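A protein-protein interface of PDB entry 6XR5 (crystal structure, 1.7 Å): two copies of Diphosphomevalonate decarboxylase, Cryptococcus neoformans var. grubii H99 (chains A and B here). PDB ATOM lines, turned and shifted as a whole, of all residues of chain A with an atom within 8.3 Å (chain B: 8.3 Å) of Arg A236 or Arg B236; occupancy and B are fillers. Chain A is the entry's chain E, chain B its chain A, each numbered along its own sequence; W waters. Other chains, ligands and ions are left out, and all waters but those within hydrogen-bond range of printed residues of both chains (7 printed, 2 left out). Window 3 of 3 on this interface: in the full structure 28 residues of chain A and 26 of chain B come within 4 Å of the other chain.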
ATOM      1  N   THR A  38      16.515  23.972  -4.857  1.00  0.00           N
ATOM      2  CA  THR A  38      16.687  23.584  -6.257  1.00  0.00           C
ATOM      3  C   THR A  38      15.944  22.311  -6.582  1.00  0.00           C
ATOM      4  O   THR A  38      15.789  21.979  -7.767  1.00  0.00           O
ATOM      5  CB  THR A  38      18.172  23.373  -6.608  1.00  0.00           C
ATOM      6  OG1 THR A  38      18.747  22.435  -5.688  1.00  0.00           O
ATOM      7  CG2 THR A  38      18.924  24.711  -6.521  1.00  0.00           C
ATOM      8  N   ASN A  39      15.472  21.597  -5.566  1.00  0.00           N
ATOM      9  CA  ASN A  39      14.763  20.351  -5.814  1.00  0.00           C
ATOM     10  C   ASN A  39      13.934  20.019  -4.579  1.00  0.00           C
ATOM     11  O   ASN A  39      14.187  20.534  -3.489  1.00  0.00           O
ATOM     12  CB  ASN A  39      15.732  19.203  -6.156  1.00  0.00           C
ATOM     13  CG  ASN A  39      16.841  19.032  -5.126  1.00  0.00           C
ATOM     14  OD1 ASN A  39      17.919  19.638  -5.251  1.00  0.00           O
ATOM     15  ND2 ASN A  39      16.578  18.230  -4.084  1.00  0.00           N
ATOM     16  N   THR A 229      28.814  20.828 -12.347  1.00  0.00           N
ATOM     17  CA  THR A 229      28.064  20.494 -13.544  1.00  0.00           C
ATOM     18  C   THR A 229      27.169  19.280 -13.286  1.00  0.00           C
ATOM     19  O   THR A 229      26.043  19.215 -13.795  1.00  0.00           O
ATOM     20  CB  THR A 229      29.005  20.244 -14.734  1.00  0.00           C
ATOM     21  OG1 THR A 229      30.003  19.281 -14.384  1.00  0.00           O
ATOM     22  CG2 THR A 229      29.692  21.555 -15.181  1.00  0.00           C
ATOM     23  N   LEU A 230      27.650  18.316 -12.487  1.00  0.00           N
ATOM     24  CA  LEU A 230      26.854  17.112 -12.273  1.00  0.00           C
ATOM     25  C   LEU A 230      25.580  17.422 -11.508  1.00  0.00           C
ATOM     26  O   LEU A 230      24.598  16.673 -11.621  1.00  0.00           O
ATOM     27  CB  LEU A 230      27.664  16.042 -11.525  1.00  0.00           C
ATOM     28  CG  LEU A 230      28.937  15.596 -12.257  1.00  0.00           C
ATOM     29  CD1 LEU A 230      29.612  14.533 -11.419  1.00  0.00           C
ATOM     30  CD2 LEU A 230      28.659  15.105 -13.702  1.00  0.00           C
ATOM     31  N   LEU A 231      25.577  18.493 -10.703  1.00  0.00           N
ATOM     32  CA  LEU A 231      24.347  18.879 -10.005  1.00  0.00           C
ATOM     33  C   LEU A 231      23.190  19.037 -10.976  1.00  0.00           C
ATOM     34  O   LEU A 231      22.051  18.674 -10.658  1.00  0.00           O
ATOM     35  CB  LEU A 231      24.552  20.172  -9.218  1.00  0.00           C
ATOM     36  CG  LEU A 231      23.255  20.664  -8.534  1.00  0.00           C
ATOM     37  CD1 LEU A 231      22.837  19.697  -7.433  1.00  0.00           C
ATOM     38  CD2 LEU A 231      23.412  22.051  -7.966  1.00  0.00           C
ATOM     39  N   GLN A 232      23.453  19.560 -12.173  1.00  0.00           N
ATOM     40  CA  GLN A 232      22.352  19.789 -13.113  1.00  0.00           C
ATOM     41  C   GLN A 232      21.677  18.481 -13.526  1.00  0.00           C
ATOM     42  O   GLN A 232      20.450  18.449 -13.745  1.00  0.00           O
ATOM     43  CB  GLN A 232      22.852  20.565 -14.333  1.00  0.00           C
ATOM     44  CG  GLN A 232      23.343  21.975 -13.935  1.00  0.00           C
ATOM     45  CD  GLN A 232      22.299  22.750 -13.111  1.00  0.00           C
ATOM     46  OE1 GLN A 232      22.568  23.202 -11.981  1.00  0.00           O
ATOM     47  NE2 GLN A 232      21.096  22.895 -13.668  1.00  0.00           N
ATOM     48  N   GLU A 233      22.433  17.385 -13.575  1.00  0.00           N
ATOM     49  CA  GLU A 233      21.813  16.087 -13.842  1.00  0.00           C
ATOM     50  C   GLU A 233      21.116  15.539 -12.598  1.00  0.00           C
ATOM     51  O   GLU A 233      20.039  14.937 -12.704  1.00  0.00           O
ATOM     52  CB  GLU A 233      22.859  15.097 -14.347  1.00  0.00           C
ATOM     53  CG  GLU A 233      22.285  13.731 -14.736  1.00  0.00           C
ATOM     54  CD  GLU A 233      21.390  13.827 -15.958  1.00  0.00           C
ATOM     55  OE1 GLU A 233      21.573  14.764 -16.764  1.00  0.00           O
ATOM     56  OE2 GLU A 233      20.510  12.968 -16.123  1.00  0.00           O
ATOM     57  N   ARG A 234      21.716  15.734 -11.423  1.00  0.00           N
ATOM     58  CA  ARG A 234      21.019  15.407 -10.176  1.00  0.00           C
ATOM     59  C   ARG A 234      19.624  16.031 -10.151  1.00  0.00           C
ATOM     60  O   ARG A 234      18.648  15.366  -9.782  1.00  0.00           O
ATOM     61  CB  ARG A 234      21.848  15.866  -8.963  1.00  0.00           C
ATOM     62  CG  ARG A 234      21.053  15.799  -7.625  1.00  0.00           C
ATOM     63  CD  ARG A 234      21.917  15.881  -6.351  1.00  0.00           C
ATOM     64  NE  ARG A 234      20.994  15.915  -5.218  1.00  0.00           N
ATOM     65  CZ  ARG A 234      20.367  14.834  -4.757  1.00  0.00           C
ATOM     66  NH1 ARG A 234      20.666  13.636  -5.267  1.00  0.00           N
ATOM     67  NH2 ARG A 234      19.454  14.953  -3.799  1.00  0.00           N
ATOM     68  N   LEU A 235      19.500  17.302 -10.556  1.00  0.00           N
ATOM     69  CA  LEU A 235      18.187  17.956 -10.491  1.00  0.00           C
ATOM     70  C   LEU A 235      17.183  17.298 -11.440  1.00  0.00           C
ATOM     71  O   LEU A 235      15.966  17.377 -11.211  1.00  0.00           O
ATOM     72  CB  LEU A 235      18.309  19.445 -10.809  1.00  0.00           C
ATOM     73  CG  LEU A 235      19.243  20.229  -9.894  1.00  0.00           C
ATOM     74  CD1 LEU A 235      19.175  21.706 -10.275  1.00  0.00           C
ATOM     75  CD2 LEU A 235      18.831  20.046  -8.461  1.00  0.00           C
ATOM     76  N   ARG A 236      17.665  16.656 -12.514  1.00  0.00           N
ATOM     77  CA  ARG A 236      16.786  15.914 -13.414  1.00  0.00           C
ATOM     78  C   ARG A 236      16.382  14.564 -12.833  1.00  0.00           C
ATOM     79  O   ARG A 236      15.298  14.056 -13.154  1.00  0.00           O
ATOM     80  CB  ARG A 236      17.469  15.692 -14.770  1.00  0.00           C
ATOM     81  CG  ARG A 236      17.755  16.964 -15.551  1.00  0.00           C
ATOM     82  CD  ARG A 236      18.565  16.714 -16.836  1.00  0.00           C
ATOM     83  NE  ARG A 236      19.175  17.980 -17.236  1.00  0.00           N
ATOM     84  CZ  ARG A 236      20.473  18.227 -17.266  1.00  0.00           C
ATOM     85  NH1 ARG A 236      21.351  17.278 -16.989  1.00  0.00           N
ATOM     86  NH2 ARG A 236      20.896  19.434 -17.607  1.00  0.00           N
ATOM     87  N   VAL A 237      17.253  13.966 -12.016  1.00  0.00           N
ATOM     88  CA  VAL A 237      17.039  12.623 -11.487  1.00  0.00           C
ATOM     89  C   VAL A 237      16.154  12.668 -10.240  1.00  0.00           C
ATOM     90  O   VAL A 237      15.352  11.750 -10.012  1.00  0.00           O
ATOM     91  CB  VAL A 237      18.406  11.970 -11.192  1.00  0.00           C
ATOM     92  CG1 VAL A 237      18.232  10.613 -10.491  1.00  0.00           C
ATOM     93  CG2 VAL A 237      19.185  11.785 -12.501  1.00  0.00           C
ATOM     94  N   VAL A 238      16.260  13.743  -9.433  1.00  0.00           N
ATOM     95  CA  VAL A 238      15.531  13.778  -8.153  1.00  0.00           C
ATOM     96  C   VAL A 238      14.028  13.597  -8.300  1.00  0.00           C
ATOM     97  O   VAL A 238      13.442  12.839  -7.505  1.00  0.00           O
ATOM     98  CB  VAL A 238      15.886  15.072  -7.378  1.00  0.00           C
ATOM     99  CG1 VAL A 238      14.874  15.314  -6.258  1.00  0.00           C
ATOM    100  CG2 VAL A 238      17.260  14.914  -6.799  1.00  0.00           C
ATOM    101  N   PRO A 239      13.329  14.257  -9.244  1.00  0.00           N
ATOM    102  CA  PRO A 239      11.877  14.019  -9.332  1.00  0.00           C
ATOM    103  C   PRO A 239      11.527  12.561  -9.537  1.00  0.00           C
ATOM    104  O   PRO A 239      10.514  12.113  -8.993  1.00  0.00           O
ATOM    105  CB  PRO A 239      11.434  14.879 -10.525  1.00  0.00           C
ATOM    106  CG  PRO A 239      12.513  15.948 -10.618  1.00  0.00           C
ATOM    107  CD  PRO A 239      13.779  15.243 -10.245  1.00  0.00           C
ATOM    108  N   LYS A 240      12.337  11.817 -10.309  1.00  0.00           N
ATOM    109  CA  LYS A 240      12.128  10.381 -10.490  1.00  0.00           C
ATOM    110  C   LYS A 240      12.276   9.637  -9.176  1.00  0.00           C
ATOM    111  O   LYS A 240      11.484   8.734  -8.878  1.00  0.00           O
ATOM    112  CB  LYS A 240      13.122   9.809 -11.509  1.00  0.00           C
ATOM    113  CG  LYS A 240      13.143  10.517 -12.863  1.00  0.00           C
ATOM    114  CD  LYS A 240      14.371  10.091 -13.674  1.00  0.00           C
ATOM    115  CE  LYS A 240      14.432  10.815 -15.006  1.00  0.00           C
ATOM    116  NZ  LYS A 240      13.232  10.512 -15.846  1.00  0.00           N
ATOM    117  N   ARG A 241      13.291  10.000  -8.377  1.00  0.00           N
ATOM    118  CA  ARG A 241      13.476   9.338  -7.093  1.00  0.00           C
ATOM    119  C   ARG A 241      12.360   9.702  -6.125  1.00  0.00           C
ATOM    120  O   ARG A 241      11.934   8.856  -5.333  1.00  0.00           O
ATOM    121  CB  ARG A 241      14.849   9.670  -6.497  1.00  0.00           C
ATOM    122  CG  ARG A 241      16.004   9.074  -7.329  1.00  0.00           C
ATOM    123  CD  ARG A 241      17.310   9.080  -6.538  1.00  0.00           C
ATOM    124  NE  ARG A 241      18.347   8.420  -7.322  1.00  0.00           N
ATOM    125  CZ  ARG A 241      19.517   8.976  -7.638  1.00  0.00           C
ATOM    126  NH1 ARG A 241      19.838  10.184  -7.185  1.00  0.00           N
ATOM    127  NH2 ARG A 241      20.363   8.292  -8.403  1.00  0.00           N
ATOM    128  N   THR B  38      34.028   5.528 -23.525  1.00  0.00           N
ATOM    129  CA  THR B  38      32.827   6.357 -23.573  1.00  0.00           C
ATOM    130  C   THR B  38      33.132   7.832 -23.791  1.00  0.00           C
ATOM    131  O   THR B  38      32.204   8.619 -24.018  1.00  0.00           O
ATOM    132  CB  THR B  38      32.027   6.201 -22.271  1.00  0.00           C
ATOM    133  OG1 THR B  38      32.874   6.543 -21.169  1.00  0.00           O
ATOM    134  CG2 THR B  38      31.498   4.757 -22.112  1.00  0.00           C
ATOM    135  N   ASN B  39      34.404   8.227 -23.729  1.00  0.00           N
ATOM    136  CA  ASN B  39      34.783   9.620 -23.903  1.00  0.00           C
ATOM    137  C   ASN B  39      36.272   9.633 -24.193  1.00  0.00           C
ATOM    138  O   ASN B  39      36.965   8.644 -23.948  1.00  0.00           O
ATOM    139  CB  ASN B  39      34.471  10.468 -22.654  1.00  0.00           C
ATOM    140  CG  ASN B  39      35.045   9.864 -21.360  1.00  0.00           C
ATOM    141  OD1 ASN B  39      34.357   9.115 -20.671  1.00  0.00           O
ATOM    142  ND2 ASN B  39      36.276  10.207 -21.030  1.00  0.00           N
ATOM    143  N   THR B 229      23.796   7.693 -12.877  1.00  0.00           N
ATOM    144  CA  THR B 229      23.054   8.679 -13.658  1.00  0.00           C
ATOM    145  C   THR B 229      23.921   9.899 -13.916  1.00  0.00           C
ATOM    146  O   THR B 229      23.852  10.506 -14.992  1.00  0.00           O
ATOM    147  CB  THR B 229      21.777   9.108 -12.937  1.00  0.00           C
ATOM    148  OG1 THR B 229      22.093   9.490 -11.591  1.00  0.00           O
ATOM    149  CG2 THR B 229      20.819   7.961 -12.887  1.00  0.00           C
ATOM    150  N   LEU B 230      24.770  10.249 -12.954  1.00  0.00           N
ATOM    151  CA  LEU B 230      25.580  11.442 -13.139  1.00  0.00           C
ATOM    152  C   LEU B 230      26.599  11.268 -14.254  1.00  0.00           C
ATOM    153  O   LEU B 230      27.005  12.256 -14.859  1.00  0.00           O
ATOM    154  CB  LEU B 230      26.281  11.819 -11.836  1.00  0.00           C
ATOM    155  CG  LEU B 230      25.268  12.125 -10.725  1.00  0.00           C
ATOM    156  CD1 LEU B 230      25.999  12.594  -9.452  1.00  0.00           C
ATOM    157  CD2 LEU B 230      24.218  13.179 -11.118  1.00  0.00           C
ATOM    158  N   LEU B 231      27.028  10.031 -14.526  1.00  0.00           N
ATOM    159  CA  LEU B 231      27.960   9.790 -15.621  1.00  0.00           C
ATOM    160  C   LEU B 231      27.458  10.391 -16.924  1.00  0.00           C
ATOM    161  O   LEU B 231      28.245  10.922 -17.707  1.00  0.00           O
ATOM    162  CB  LEU B 231      28.209   8.277 -15.787  1.00  0.00           C
ATOM    163  CG  LEU B 231      29.177   8.008 -16.970  1.00  0.00           C
ATOM    164  CD1 LEU B 231      30.618   8.494 -16.752  1.00  0.00           C
ATOM    165  CD2 LEU B 231      29.164   6.544 -17.301  1.00  0.00           C
ATOM    166  N   GLN B 232      26.145  10.365 -17.164  1.00  0.00           N
ATOM    167  CA  GLN B 232      25.671  10.848 -18.457  1.00  0.00           C
ATOM    168  C   GLN B 232      25.966  12.338 -18.639  1.00  0.00           C
ATOM    169  O   GLN B 232      26.244  12.787 -19.764  1.00  0.00           O
ATOM    170  CB  GLN B 232      24.190  10.509 -18.637  1.00  0.00           C
ATOM    171  CG  GLN B 232      23.957   8.976 -18.746  1.00  0.00           C
ATOM    172  CD  GLN B 232      24.866   8.280 -19.799  1.00  0.00           C
ATOM    173  OE1 GLN B 232      24.869   8.636 -20.991  1.00  0.00           O
ATOM    174  NE2 GLN B 232      25.664   7.305 -19.347  1.00  0.00           N
ATOM    175  N   GLU B 233      25.968  13.111 -17.545  1.00  0.00           N
ATOM    176  CA  GLU B 233      26.354  14.514 -17.636  1.00  0.00           C
ATOM    177  C   GLU B 233      27.856  14.669 -17.757  1.00  0.00           C
ATOM    178  O   GLU B 233      28.329  15.569 -18.466  1.00  0.00           O
ATOM    179  CB  GLU B 233      25.836  15.296 -16.426  1.00  0.00           C
ATOM    180  CG  GLU B 233      26.139  16.787 -16.475  1.00  0.00           C
ATOM    181  CD  GLU B 233      25.389  17.524 -17.591  1.00  0.00           C
ATOM    182  OE1 GLU B 233      24.373  17.001 -18.100  1.00  0.00           O
ATOM    183  OE2 GLU B 233      25.850  18.617 -17.967  1.00  0.00           O
ATOM    184  N   ARG B 234      28.624  13.847 -17.030  1.00  0.00           N
ATOM    185  CA  ARG B 234      30.076  13.849 -17.231  1.00  0.00           C
ATOM    186  C   ARG B 234      30.421  13.668 -18.707  1.00  0.00           C
ATOM    187  O   ARG B 234      31.296  14.359 -19.232  1.00  0.00           O
ATOM    188  CB  ARG B 234      30.741  12.764 -16.372  1.00  0.00           C
ATOM    189  CG  ARG B 234      32.211  12.497 -16.766  1.00  0.00           C
ATOM    190  CD  ARG B 234      32.979  11.595 -15.787  1.00  0.00           C
ATOM    191  NE  ARG B 234      34.290  11.405 -16.369  1.00  0.00           N
ATOM    192  CZ  ARG B 234      35.224  12.346 -16.382  1.00  0.00           C
ATOM    193  NH1 ARG B 234      35.005  13.503 -15.764  1.00  0.00           N
ATOM    194  NH2 ARG B 234      36.363  12.142 -17.035  1.00  0.00           N
ATOM    195  N   LEU B 235      29.738  12.751 -19.396  1.00  0.00           N
ATOM    196  CA  LEU B 235      30.046  12.524 -20.811  1.00  0.00           C
ATOM    197  C   LEU B 235      29.730  13.740 -21.680  1.00  0.00           C
ATOM    198  O   LEU B 235      30.355  13.920 -22.740  1.00  0.00           O
ATOM    199  CB  LEU B 235      29.304  11.282 -21.308  1.00  0.00           C
ATOM    200  CG  LEU B 235      29.706  10.002 -20.566  1.00  0.00           C
ATOM    201  CD1 LEU B 235      28.863   8.847 -21.067  1.00  0.00           C
ATOM    202  CD2 LEU B 235      31.182   9.673 -20.678  1.00  0.00           C
ATOM    203  N   ARG B 236      28.792  14.599 -21.260  1.00  0.00           N
ATOM    204  CA  ARG B 236      28.549  15.839 -21.996  1.00  0.00           C
ATOM    205  C   ARG B 236      29.586  16.894 -21.671  1.00  0.00           C
ATOM    206  O   ARG B 236      29.832  17.779 -22.498  1.00  0.00           O
ATOM    207  CB  ARG B 236      27.162  16.424 -21.671  1.00  0.00           C
ATOM    208  CG  ARG B 236      26.022  15.517 -22.034  1.00  0.00           C
ATOM    209  CD  ARG B 236      24.663  16.045 -21.538  1.00  0.00           C
ATOM    210  NE  ARG B 236      23.745  14.928 -21.551  1.00  0.00           N
ATOM    211  CZ  ARG B 236      23.146  14.417 -20.487  1.00  0.00           C
ATOM    212  NH1 ARG B 236      23.300  14.960 -19.281  1.00  0.00           N
ATOM    213  NH2 ARG B 236      22.351  13.371 -20.645  1.00  0.00           N
ATOM    214  N   VAL B 237      30.149  16.854 -20.463  1.00  0.00           N
ATOM    215  CA  VAL B 237      31.105  17.894 -20.048  1.00  0.00           C
ATOM    216  C   VAL B 237      32.508  17.610 -20.573  1.00  0.00           C
ATOM    217  O   VAL B 237      33.263  18.543 -20.856  1.00  0.00           O
ATOM    218  CB  VAL B 237      31.116  18.025 -18.512  1.00  0.00           C
ATOM    219  CG1 VAL B 237      32.187  19.039 -18.054  1.00  0.00           C
ATOM    220  CG2 VAL B 237      29.753  18.498 -18.031  1.00  0.00           C
ATOM    221  N   VAL B 238      32.901  16.347 -20.669  1.00  0.00           N
ATOM    222  CA  VAL B 238      34.282  16.001 -21.028  1.00  0.00           C
ATOM    223  C   VAL B 238      34.705  16.643 -22.353  1.00  0.00           C
ATOM    224  O   VAL B 238      35.834  17.161 -22.421  1.00  0.00           O
ATOM    225  CB  VAL B 238      34.495  14.476 -21.040  1.00  0.00           C
ATOM    226  CG1 VAL B 238      35.805  14.089 -21.777  1.00  0.00           C
ATOM    227  CG2 VAL B 238      34.537  13.930 -19.594  1.00  0.00           C
ATOM    228  N   PRO B 239      33.889  16.660 -23.423  1.00  0.00           N
ATOM    229  CA  PRO B 239      34.402  17.257 -24.684  1.00  0.00           C
ATOM    230  C   PRO B 239      34.772  18.715 -24.517  1.00  0.00           C
ATOM    231  O   PRO B 239      35.739  19.196 -25.130  1.00  0.00           O
ATOM    232  CB  PRO B 239      33.232  17.087 -25.673  1.00  0.00           C
ATOM    233  CG  PRO B 239      32.467  15.914 -25.161  1.00  0.00           C
ATOM    234  CD  PRO B 239      32.612  15.940 -23.646  1.00  0.00           C
ATOM    235  N   LYS B 240      34.005  19.437 -23.694  1.00  0.00           N
ATOM    236  CA  LYS B 240      34.324  20.830 -23.400  1.00  0.00           C
ATOM    237  C   LYS B 240      35.654  20.947 -22.666  1.00  0.00           C
ATOM    238  O   LYS B 240      36.433  21.868 -22.935  1.00  0.00           O
ATOM    239  CB  LYS B 240      33.200  21.461 -22.567  1.00  0.00           C
ATOM    240  CG  LYS B 240      31.820  21.353 -23.176  1.00  0.00           C
ATOM    241  CD  LYS B 240      30.762  21.867 -22.187  1.00  0.00           C
ATOM    242  CE  LYS B 240      29.366  21.621 -22.712  1.00  0.00           C
ATOM    243  NZ  LYS B 240      29.094  22.461 -23.914  1.00  0.00           N
ATOM    244  N   ARG B 241      35.909  20.063 -21.690  1.00  0.00           N
ATOM    245  CA  ARG B 241      37.185  20.111 -20.985  1.00  0.00           C
ATOM    246  C   ARG B 241      38.339  19.696 -21.892  1.00  0.00           C
ATOM    247  O   ARG B 241      39.443  20.238 -21.774  1.00  0.00           O
ATOM    248  CB  ARG B 241      37.162  19.227 -19.741  1.00  0.00           C
ATOM    249  CG  ARG B 241      36.158  19.715 -18.727  1.00  0.00           C
ATOM    250  CD  ARG B 241      36.349  18.972 -17.401  1.00  0.00           C
ATOM    251  NE  ARG B 241      35.448  19.527 -16.382  1.00  0.00           N
ATOM    252  CZ  ARG B 241      34.668  18.809 -15.570  1.00  0.00           C
ATOM    253  NH1 ARG B 241      34.659  17.479 -15.589  1.00  0.00           N
ATOM    254  NH2 ARG B 241      33.877  19.457 -14.730  1.00  0.00           N
HETATM  255  O   HOH W   1      23.183  20.803 -17.577  1.00  0.00           O
HETATM  256  O   HOH W   2      31.707  20.148 -12.462  1.00  0.00           O
HETATM  257  O   HOH W   3      22.606  10.474  -9.017  1.00  0.00           O
HETATM  258  O   HOH W   4      22.898   7.425 -10.033  1.00  0.00           O
HETATM  259  O   HOH W   5      31.932  17.130 -13.629  1.00  0.00           O
HETATM  260  O   HOH W   6      19.739  13.968 -18.638  1.00  0.00           O
HETATM  261  O   HOH W   7      21.400  10.180 -16.466  1.00  0.00           O
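The side-chain carboxylate (OE1) of Glu B233 lies within salt-bridge range of the guanidinium group (NH1) of Arg A236, 3.2 Å away.
OE1 of Glu A233 is in salt-bridge range of NH1 of Arg B236, at 3.1 Å.
The side-chain carboxylate of Glu B233 is in salt-bridge range of the guanidinium group of Arg B236, at 2.6 Å.
The side-chain carboxylate (OE1) of Glu A233 is in salt-bridge range of the guanidinium group (NH1) of Arg A236 (2.5 Å).
Among the printed residues, merely in contact across the chains: Leu A230 with Leu B230 (3.5 Å), Leu A230 with Arg B234 (3.6 Å), Arg A234 with Leu B230 (3.6 Å), Glu A233 with Thr B229 (3.6 Å), Thr A229 with Glu B233 (3.6 Å), Glu A233 with Glu B233 (3.6 Å), Thr A229 with Val B237 (3.7 Å), Val A237 with Thr B229 (3.8 Å), Arg A236 with Arg B236 (3.8 Å), Arg A241 with Thr B229 (3.8 Å), Thr A229 with Arg B241 (3.9 Å), Leu A230 with Glu B233 (3.9 Å) and Glu A233 with Leu B230 (3.99 Å).
Of chain B, only Glu B233 and Arg B236 come within 4 Å of Arg A236.
Val A238 touches none of the printed residues of chain B.
Asn B39 touches none of the printed residues of chain A.
Printed residues of chain A within 4 Å of Arg B234: Leu A230.
Arg B236 touches just these residues of chain A: Glu A233 and Arg A236.
Of the printed residues of chain A, Val B237 touches Thr A229.
Hydrophobic or aromatic side chains of chain A within 4 Å of the printed part of chain B: Leu A230 and Val A237.
Of the 15 printed residues of chain B, 7 touch a printed residue of chain A.
Printed residues of chain B that touch a printed residue of chain A: Thr B229, Leu B230, Glu B233, Arg B234, Arg B236, Val B237 and Arg B241.
Hydrophobic or aromatic side chains of chain B that line the printed part of chain A: Leu B230 and Val B237.
Thr A229 touches Glu B233, and with the chains exchanged Glu A233 touches Thr B229.
Leu A230 touches Arg B234, and with the chains exchanged Arg A234 touches Leu B230.
Glu B233 touches its own counterpart, Glu A233.
Glu A233 touches Arg B236, and with the chains exchanged Arg A236 touches Glu B233.
Water W4 lies within hydrogen-bond range of the side-chain hydroxyl (OG1) of Thr B229 (2.7 Å) and the guanidinium group (NH2) of Arg A241 (3.1 Å).
Water W2 bridges the side-chain hydroxyl (OG1) of Thr A229 and the guanidinium group (NH2) of Arg B241.
Water W6 bridges the side-chain carboxylate of Glu A233 (2.7 Å) and the guanidinium group of Arg B236 (3.3 Å).
Water W3 bridges the side-chain hydroxyl (OG1) of Thr B229 (2.8 Å) and the guanidinium group (NH2) of Arg A241 (3.2 Å).
Water W7 lies within hydrogen-bond range of O of Thr B229 (2.9 Å) and OE2 of Glu A233 (2.9 Å).
Water W5 lies within hydrogen-bond range of OG1 of Thr A229 and NH2 of Arg B241.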
